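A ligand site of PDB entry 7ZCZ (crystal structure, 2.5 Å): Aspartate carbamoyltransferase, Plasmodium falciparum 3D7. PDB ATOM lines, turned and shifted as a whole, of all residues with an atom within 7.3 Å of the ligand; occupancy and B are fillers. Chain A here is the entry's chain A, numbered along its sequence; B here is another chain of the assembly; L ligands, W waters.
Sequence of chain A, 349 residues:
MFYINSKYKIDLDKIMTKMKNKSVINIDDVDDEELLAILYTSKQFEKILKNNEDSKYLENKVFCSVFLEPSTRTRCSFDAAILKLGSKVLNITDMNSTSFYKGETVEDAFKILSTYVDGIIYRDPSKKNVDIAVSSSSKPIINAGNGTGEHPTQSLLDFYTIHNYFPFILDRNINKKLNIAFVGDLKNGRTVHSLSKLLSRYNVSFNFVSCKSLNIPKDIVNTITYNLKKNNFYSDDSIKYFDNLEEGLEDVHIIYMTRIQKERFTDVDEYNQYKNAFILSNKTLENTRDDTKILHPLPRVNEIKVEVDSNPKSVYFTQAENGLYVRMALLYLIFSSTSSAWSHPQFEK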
ATOM      1  N   CYS A  64      18.487  -8.014 -24.116  1.00  0.00           N
ATOM      2  CA  CYS A  64      19.496  -7.953 -23.033  1.00  0.00           C
ATOM      3  C   CYS A  64      20.319  -6.670 -23.211  1.00  0.00           C
ATOM      4  O   CYS A  64      20.768  -6.375 -24.322  1.00  0.00           O
ATOM      5  CB  CYS A  64      20.424  -9.143 -23.052  1.00  0.00           C
ATOM      6  SG  CYS A  64      21.533  -9.101 -21.639  1.00  0.00           S
ATOM      7  N   VAL A  66      23.728  -5.084 -21.878  1.00  0.00           N
ATOM      8  CA  VAL A  66      25.026  -5.361 -21.221  1.00  0.00           C
ATOM      9  C   VAL A  66      25.836  -4.074 -21.169  1.00  0.00           C
ATOM     10  O   VAL A  66      26.207  -3.588 -22.224  1.00  0.00           O
ATOM     11  CB  VAL A  66      25.766  -6.464 -21.983  1.00  0.00           C
ATOM     12  CG1 VAL A  66      27.022  -6.943 -21.264  1.00  0.00           C
ATOM     13  CG2 VAL A  66      24.838  -7.641 -22.236  1.00  0.00           C
ATOM     14  N   ILE A  92      22.407  -6.297 -17.576  1.00  0.00           N
ATOM     15  CA  ILE A  92      23.699  -6.638 -16.905  1.00  0.00           C
ATOM     16  C   ILE A  92      24.495  -5.353 -16.742  1.00  0.00           C
ATOM     17  O   ILE A  92      24.846  -4.788 -17.766  1.00  0.00           O
ATOM     18  CB  ILE A  92      24.445  -7.671 -17.739  1.00  0.00           C
ATOM     19  CG1 ILE A  92      23.674  -8.988 -17.825  1.00  0.00           C
ATOM     20  CG2 ILE A  92      25.837  -7.858 -17.232  1.00  0.00           C
ATOM     21  CD1 ILE A  92      23.996  -9.772 -19.110  1.00  0.00           C
ATOM     22  N   MET A  95      29.153  -4.058 -13.445  1.00  0.00           N
ATOM     23  CA  MET A  95      30.348  -4.921 -13.679  1.00  0.00           C
ATOM     24  C   MET A  95      31.227  -4.135 -14.662  1.00  0.00           C
ATOM     25  O   MET A  95      30.682  -3.180 -15.318  1.00  0.00           O
ATOM     26  CB  MET A  95      29.961  -6.274 -14.283  1.00  0.00           C
ATOM     27  CG  MET A  95      28.956  -7.028 -13.421  1.00  0.00           C
ATOM     28  SD  MET A  95      28.487  -8.700 -13.923  1.00  0.00           S
ATOM     29  CE  MET A  95      26.832  -8.799 -13.217  1.00  0.00           C
ATOM     30  N   SER A  99      35.335  -8.644 -14.611  1.00  0.00           N
ATOM     31  CA  SER A  99      34.419  -9.237 -13.596  1.00  0.00           C
ATOM     32  C   SER A  99      33.242  -9.984 -14.277  1.00  0.00           C
ATOM     33  O   SER A  99      32.741 -10.943 -13.660  1.00  0.00           O
ATOM     34  CB  SER A  99      33.959  -8.200 -12.593  1.00  0.00           C
ATOM     35  OG  SER A  99      32.830  -7.468 -13.070  1.00  0.00           O
ATOM     36  N   PHE A 100      32.802  -9.564 -15.470  1.00  0.00           N
ATOM     37  CA  PHE A 100      31.692 -10.200 -16.243  1.00  0.00           C
ATOM     38  C   PHE A 100      32.205 -11.435 -16.990  1.00  0.00           C
ATOM     39  O   PHE A 100      31.543 -12.464 -16.923  1.00  0.00           O
ATOM     40  CB  PHE A 100      31.030  -9.193 -17.189  1.00  0.00           C
ATOM     41  CG  PHE A 100      30.069  -9.750 -18.216  1.00  0.00           C
ATOM     42  CD1 PHE A 100      28.765 -10.079 -17.874  1.00  0.00           C
ATOM     43  CD2 PHE A 100      30.410  -9.870 -19.561  1.00  0.00           C
ATOM     44  CE1 PHE A 100      27.871 -10.540 -18.819  1.00  0.00           C
ATOM     45  CE2 PHE A 100      29.503 -10.330 -20.506  1.00  0.00           C
ATOM     46  CZ  PHE A 100      28.234 -10.657 -20.141  1.00  0.00           C
ATOM     47  N   TYR A 101      33.346 -11.357 -17.688  1.00  0.00           N
ATOM     48  CA  TYR A 101      33.961 -12.500 -18.435  1.00  0.00           C
ATOM     49  C   TYR A 101      34.866 -13.296 -17.466  1.00  0.00           C
ATOM     50  O   TYR A 101      36.063 -13.517 -17.776  1.00  0.00           O
ATOM     51  CB  TYR A 101      34.744 -12.006 -19.657  1.00  0.00           C
ATOM     52  CG  TYR A 101      33.901 -11.293 -20.692  1.00  0.00           C
ATOM     53  CD1 TYR A 101      32.910 -11.959 -21.390  1.00  0.00           C
ATOM     54  CD2 TYR A 101      34.069  -9.941 -20.929  1.00  0.00           C
ATOM     55  CE1 TYR A 101      32.119 -11.304 -22.330  1.00  0.00           C
ATOM     56  CE2 TYR A 101      33.281  -9.262 -21.853  1.00  0.00           C
ATOM     57  CZ  TYR A 101      32.309  -9.950 -22.562  1.00  0.00           C
ATOM     58  OH  TYR A 101      31.548  -9.273 -23.469  1.00  0.00           O
ATOM     59  N   LYS A 102      34.327 -13.690 -16.297  1.00  0.00           N
ATOM     60  CA  LYS A 102      35.104 -14.361 -15.218  1.00  0.00           C
ATOM     61  C   LYS A 102      35.974 -15.448 -15.877  1.00  0.00           C
ATOM     62  O   LYS A 102      35.700 -16.648 -15.703  1.00  0.00           O
ATOM     63  CB  LYS A 102      34.145 -14.892 -14.130  1.00  0.00           C
ATOM     64  CG  LYS A 102      33.647 -13.953 -13.012  1.00  0.00           C
ATOM     65  CD  LYS A 102      34.635 -13.057 -12.151  1.00  0.00           C
ATOM     66  CE  LYS A 102      36.093 -13.464 -12.062  1.00  0.00           C
ATOM     67  NZ  LYS A 102      36.380 -14.262 -10.850  1.00  0.00           N
ATOM     68  N   GLU A 104      35.905 -16.524 -18.884  1.00  0.00           N
ATOM     69  CA  GLU A 104      35.234 -17.159 -20.055  1.00  0.00           C
ATOM     70  C   GLU A 104      35.414 -16.245 -21.273  1.00  0.00           C
ATOM     71  O   GLU A 104      35.479 -15.022 -21.070  1.00  0.00           O
ATOM     72  CB  GLU A 104      33.749 -17.377 -19.774  1.00  0.00           C
ATOM     73  CG  GLU A 104      32.927 -17.748 -21.001  1.00  0.00           C
ATOM     74  CD  GLU A 104      31.442 -18.029 -20.734  1.00  0.00           C
ATOM     75  OE1 GLU A 104      30.765 -17.129 -20.144  1.00  0.00           O
ATOM     76  OE2 GLU A 104      30.968 -19.139 -21.106  1.00  0.00           O
ATOM     77  N   THR A 105      35.468 -16.805 -22.484  1.00  0.00           N
ATOM     78  CA  THR A 105      35.708 -16.060 -23.747  1.00  0.00           C
ATOM     79  C   THR A 105      34.489 -15.184 -24.068  1.00  0.00           C
ATOM     80  O   THR A 105      33.343 -15.559 -23.749  1.00  0.00           O
ATOM     81  CB  THR A 105      36.015 -16.994 -24.933  1.00  0.00           C
ATOM     82  OG1 THR A 105      34.901 -17.837 -25.222  1.00  0.00           O
ATOM     83  CG2 THR A 105      37.233 -17.868 -24.739  1.00  0.00           C
ATOM     84  N   ASP A 108      32.136 -17.284 -26.395  1.00  0.00           N
ATOM     85  CA  ASP A 108      31.218 -18.224 -25.694  1.00  0.00           C
ATOM     86  C   ASP A 108      30.075 -17.430 -25.070  1.00  0.00           C
ATOM     87  O   ASP A 108      28.933 -17.867 -25.169  1.00  0.00           O
ATOM     88  CB  ASP A 108      31.929 -19.039 -24.595  1.00  0.00           C
ATOM     89  CG  ASP A 108      32.874 -20.104 -25.135  1.00  0.00           C
ATOM     90  OD1 ASP A 108      32.892 -20.253 -26.348  1.00  0.00           O
ATOM     91  OD2 ASP A 108      33.556 -20.773 -24.326  1.00  0.00           O
ATOM     92  N   ALA A 109      30.374 -16.309 -24.431  1.00  0.00           N
ATOM     93  CA  ALA A 109      29.379 -15.536 -23.652  1.00  0.00           C
ATOM     94  C   ALA A 109      28.258 -15.044 -24.581  1.00  0.00           C
ATOM     95  O   ALA A 109      27.065 -15.190 -24.219  1.00  0.00           O
ATOM     96  CB  ALA A 109      30.078 -14.404 -22.932  1.00  0.00           C
ATOM     97  N   PHE A 110      28.610 -14.523 -25.742  1.00  0.00           N
ATOM     98  CA  PHE A 110      27.637 -13.912 -26.678  1.00  0.00           C
ATOM     99  C   PHE A 110      26.963 -15.005 -27.475  1.00  0.00           C
ATOM    100  O   PHE A 110      25.808 -14.809 -27.875  1.00  0.00           O
ATOM    101  CB  PHE A 110      28.282 -12.855 -27.589  1.00  0.00           C
ATOM    102  CG  PHE A 110      28.158 -11.490 -26.986  1.00  0.00           C
ATOM    103  CD1 PHE A 110      29.039 -11.088 -26.003  1.00  0.00           C
ATOM    104  CD2 PHE A 110      27.104 -10.672 -27.295  1.00  0.00           C
ATOM    105  CE1 PHE A 110      28.907  -9.865 -25.370  1.00  0.00           C
ATOM    106  CE2 PHE A 110      26.965  -9.452 -26.650  1.00  0.00           C
ATOM    107  CZ  PHE A 110      27.858  -9.068 -25.690  1.00  0.00           C
ATOM    108  N   LYS A 111      27.656 -16.115 -27.698  1.00  0.00           N
ATOM    109  CA  LYS A 111      27.046 -17.284 -28.388  1.00  0.00           C
ATOM    110  C   LYS A 111      25.826 -17.717 -27.534  1.00  0.00           C
ATOM    111  O   LYS A 111      24.754 -17.871 -28.109  1.00  0.00           O
ATOM    112  CB  LYS A 111      28.137 -18.333 -28.613  1.00  0.00           C
ATOM    113  CG  LYS A 111      27.792 -19.456 -29.586  1.00  0.00           C
ATOM    114  CD  LYS A 111      29.017 -20.077 -30.271  1.00  0.00           C
ATOM    115  CE  LYS A 111      28.689 -21.325 -31.059  1.00  0.00           C
ATOM    116  NZ  LYS A 111      27.444 -21.146 -31.850  1.00  0.00           N
ATOM    117  N   ILE A 112      26.010 -17.813 -26.219  1.00  0.00           N
ATOM    118  CA  ILE A 112      24.981 -18.335 -25.259  1.00  0.00           C
ATOM    119  C   ILE A 112      23.892 -17.271 -25.064  1.00  0.00           C
ATOM    120  O   ILE A 112      22.680 -17.568 -25.158  1.00  0.00           O
ATOM    121  CB  ILE A 112      25.614 -18.694 -23.897  1.00  0.00           C
ATOM    122  CG1 ILE A 112      26.585 -19.875 -23.981  1.00  0.00           C
ATOM    123  CG2 ILE A 112      24.539 -18.977 -22.883  1.00  0.00           C
ATOM    124  CD1 ILE A 112      27.600 -19.887 -22.859  1.00  0.00           C
ATOM    125  N   LEU A 113      24.305 -16.057 -24.731  1.00  0.00           N
ATOM    126  CA  LEU A 113      23.367 -14.982 -24.389  1.00  0.00           C
ATOM    127  C   LEU A 113      22.456 -14.648 -25.590  1.00  0.00           C
ATOM    128  O   LEU A 113      21.282 -14.326 -25.360  1.00  0.00           O
ATOM    129  CB  LEU A 113      24.193 -13.780 -23.922  1.00  0.00           C
ATOM    130  CG  LEU A 113      23.353 -12.589 -23.516  1.00  0.00           C
ATOM    131  CD1 LEU A 113      22.443 -12.931 -22.328  1.00  0.00           C
ATOM    132  CD2 LEU A 113      24.252 -11.422 -23.199  1.00  0.00           C
ATOM    133  N   SER A 114      22.946 -14.774 -26.827  1.00  0.00           N
ATOM    134  CA  SER A 114      22.112 -14.513 -28.014  1.00  0.00           C
ATOM    135  C   SER A 114      21.065 -15.609 -28.212  1.00  0.00           C
ATOM    136  O   SER A 114      20.085 -15.348 -28.929  1.00  0.00           O
ATOM    137  CB  SER A 114      22.920 -14.258 -29.261  1.00  0.00           C
ATOM    138  OG  SER A 114      23.751 -15.328 -29.643  1.00  0.00           O
ATOM    139  N   THR A 115      21.169 -16.768 -27.547  1.00  0.00           N
ATOM    140  CA  THR A 115      20.088 -17.787 -27.586  1.00  0.00           C
ATOM    141  C   THR A 115      18.920 -17.396 -26.666  1.00  0.00           C
ATOM    142  O   THR A 115      17.875 -17.994 -26.828  1.00  0.00           O
ATOM    143  CB  THR A 115      20.621 -19.179 -27.262  1.00  0.00           C
ATOM    144  OG1 THR A 115      21.002 -19.293 -25.879  1.00  0.00           O
ATOM    145  CG2 THR A 115      21.791 -19.552 -28.142  1.00  0.00           C
ATOM    146  N   TYR A 116      19.070 -16.424 -25.764  1.00  0.00           N
ATOM    147  CA  TYR A 116      18.067 -16.086 -24.728  1.00  0.00           C
ATOM    148  C   TYR A 116      17.173 -14.946 -25.175  1.00  0.00           C
ATOM    149  O   TYR A 116      16.059 -14.819 -24.699  1.00  0.00           O
ATOM    150  CB  TYR A 116      18.747 -15.643 -23.427  1.00  0.00           C
ATOM    151  CG  TYR A 116      19.523 -16.708 -22.687  1.00  0.00           C
ATOM    152  CD1 TYR A 116      19.437 -18.047 -23.041  1.00  0.00           C
ATOM    153  CD2 TYR A 116      20.334 -16.364 -21.626  1.00  0.00           C
ATOM    154  CE1 TYR A 116      20.122 -19.029 -22.321  1.00  0.00           C
ATOM    155  CE2 TYR A 116      21.069 -17.333 -20.948  1.00  0.00           C
ATOM    156  CZ  TYR A 116      20.947 -18.679 -21.266  1.00  0.00           C
ATOM    157  OH  TYR A 116      21.634 -19.637 -20.548  1.00  0.00           O
ATOM    158  N   SER B  71      25.783 -15.472 -10.661  1.00  0.00           N
ATOM    159  CA  SER B  71      25.580 -16.608 -11.583  1.00  0.00           C
ATOM    160  C   SER B  71      24.837 -16.020 -12.780  1.00  0.00           C
ATOM    161  O   SER B  71      23.647 -16.366 -12.982  1.00  0.00           O
ATOM    162  CB  SER B  71      24.872 -17.780 -10.908  1.00  0.00           C
ATOM    163  OG  SER B  71      24.783 -18.909 -11.774  1.00  0.00           O
ATOM    164  N   THR B  72      25.527 -15.088 -13.456  1.00  0.00           N
ATOM    165  CA  THR B  72      24.954 -14.177 -14.479  1.00  0.00           C
ATOM    166  C   THR B  72      24.264 -14.996 -15.595  1.00  0.00           C
ATOM    167  O   THR B  72      23.115 -14.672 -15.961  1.00  0.00           O
ATOM    168  CB  THR B  72      26.030 -13.172 -14.931  1.00  0.00           C
ATOM    169  OG1 THR B  72      26.299 -12.227 -13.903  1.00  0.00           O
ATOM    170  CG2 THR B  72      25.582 -12.343 -16.109  1.00  0.00           C
ATOM    171  N   ARG B  73      24.882 -16.052 -16.132  1.00  0.00           N
ATOM    172  CA  ARG B  73      24.235 -16.804 -17.223  1.00  0.00           C
ATOM    173  C   ARG B  73      22.875 -17.329 -16.715  1.00  0.00           C
ATOM    174  O   ARG B  73      21.895 -17.201 -17.472  1.00  0.00           O
ATOM    175  CB  ARG B  73      25.137 -17.933 -17.736  1.00  0.00           C
ATOM    176  CG  ARG B  73      24.449 -18.879 -18.736  1.00  0.00           C
ATOM    177  CD  ARG B  73      25.266 -20.154 -19.057  1.00  0.00           C
ATOM    178  NE  ARG B  73      26.701 -19.945 -19.372  1.00  0.00           N
ATOM    179  CZ  ARG B  73      27.706 -19.769 -18.484  1.00  0.00           C
ATOM    180  NH1 ARG B  73      28.928 -19.480 -18.905  1.00  0.00           N
ATOM    181  NH2 ARG B  73      27.500 -19.846 -17.178  1.00  0.00           N
ATOM    182  N   THR B  74      22.831 -17.959 -15.541  1.00  0.00           N
ATOM    183  CA  THR B  74      21.625 -18.655 -15.003  1.00  0.00           C
ATOM    184  C   THR B  74      20.542 -17.599 -14.704  1.00  0.00           C
ATOM    185  O   THR B  74      19.380 -17.809 -15.086  1.00  0.00           O
ATOM    186  CB  THR B  74      21.934 -19.512 -13.765  1.00  0.00           C
ATOM    187  OG1 THR B  74      22.983 -20.407 -14.123  1.00  0.00           O
ATOM    188  CG2 THR B  74      20.755 -20.354 -13.314  1.00  0.00           C
ATOM    189  N   CYS B  76      20.169 -14.615 -16.115  1.00  0.00           N
ATOM    190  CA  CYS B  76      19.754 -14.080 -17.435  1.00  0.00           C
ATOM    191  C   CYS B  76      18.778 -15.084 -18.060  1.00  0.00           C
ATOM    192  O   CYS B  76      17.775 -14.705 -18.679  1.00  0.00           O
ATOM    193  CB  CYS B  76      20.968 -13.766 -18.296  1.00  0.00           C
ATOM    194  SG  CYS B  76      21.805 -12.261 -17.734  1.00  0.00           S
ATOM    195  N   SER B  77      19.031 -16.350 -17.854  1.00  0.00           N
ATOM    196  CA  SER B  77      18.260 -17.427 -18.512  1.00  0.00           C
ATOM    197  C   SER B  77      16.861 -17.384 -17.903  1.00  0.00           C
ATOM    198  O   SER B  77      15.852 -17.461 -18.633  1.00  0.00           O
ATOM    199  CB  SER B  77      18.975 -18.758 -18.315  1.00  0.00           C
ATOM    200  OG  SER B  77      18.238 -19.786 -18.924  1.00  0.00           O
ATOM    201  N   PRO B 299      30.444 -22.519 -17.875  1.00  0.00           N
ATOM    202  CA  PRO B 299      31.436 -22.219 -18.894  1.00  0.00           C
ATOM    203  C   PRO B 299      32.528 -23.262 -18.997  1.00  0.00           C
ATOM    204  O   PRO B 299      32.794 -23.909 -18.017  1.00  0.00           O
ATOM    205  CB  PRO B 299      32.095 -20.912 -18.395  1.00  0.00           C
ATOM    206  CG  PRO B 299      32.006 -21.037 -16.891  1.00  0.00           C
ATOM    207  CD  PRO B 299      30.695 -21.760 -16.647  1.00  0.00           C
HETATM  208  N1  LIG L   1      29.713 -15.195 -17.273  1.00  0.00           N
HETATM  209  C1  LIG L   1      29.581 -14.342 -18.461  1.00  0.00           C
HETATM  210  C2  LIG L   1      28.242 -14.663 -19.073  1.00  0.00           C
HETATM  211  C3  LIG L   1      28.056 -15.712 -19.947  1.00  0.00           C
HETATM  212  C4  LIG L   1      26.815 -15.986 -20.469  1.00  0.00           C
HETATM  213  C5  LIG L   1      25.741 -15.203 -20.094  1.00  0.00           C
HETATM  214  C6  LIG L   1      25.904 -14.171 -19.213  1.00  0.00           C
HETATM  215  C7  LIG L   1      27.150 -13.911 -18.690  1.00  0.00           C
HETATM  216 CL1  LIG L   1      24.151 -15.544 -20.730  1.00  0.00          CL
HETATM  217  O   HOH W   1      28.362 -16.473 -15.384  1.00  0.00           O
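The side-chain carboxylate of Glu 104 lies within salt-bridge range of a nitrogen (N1) of the ligand, at 3.6 Å. The backbone carbonyl oxygen (O) of Phe 100 lies close to a nitrogen (N1) of the ligand.
Ala 109 touches the ligand. Leu 113 touches the ligand. CE2 of Tyr 116 touches CL1 of the ligand, at 3.6 Å. Thr 72 of chain B touches the ligand. Arg 73 of chain B touches the ligand. Hydrophobic or aromatic side chains within 4 Å of the ligand: Phe 100, Ala 109, Leu 113 and Tyr 116. Seven residues have an atom within 4 Å of the ligand: Phe 100, Glu 104, Ala 109, Leu 113, Tyr 116, Thr 72 of chain B and Arg 73 of chain B.
The backbone carbonyl oxygen (O) of Thr 72 of chain B lies within hydrogen-bond range of the side-chain sulfur (SG) of Cys 76 of chain B, 3.3 Å away. The guanidinium group (NH1) of Arg 73 of chain B lies within salt-bridge range of the side-chain carboxylate (OE2) of Glu 104.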
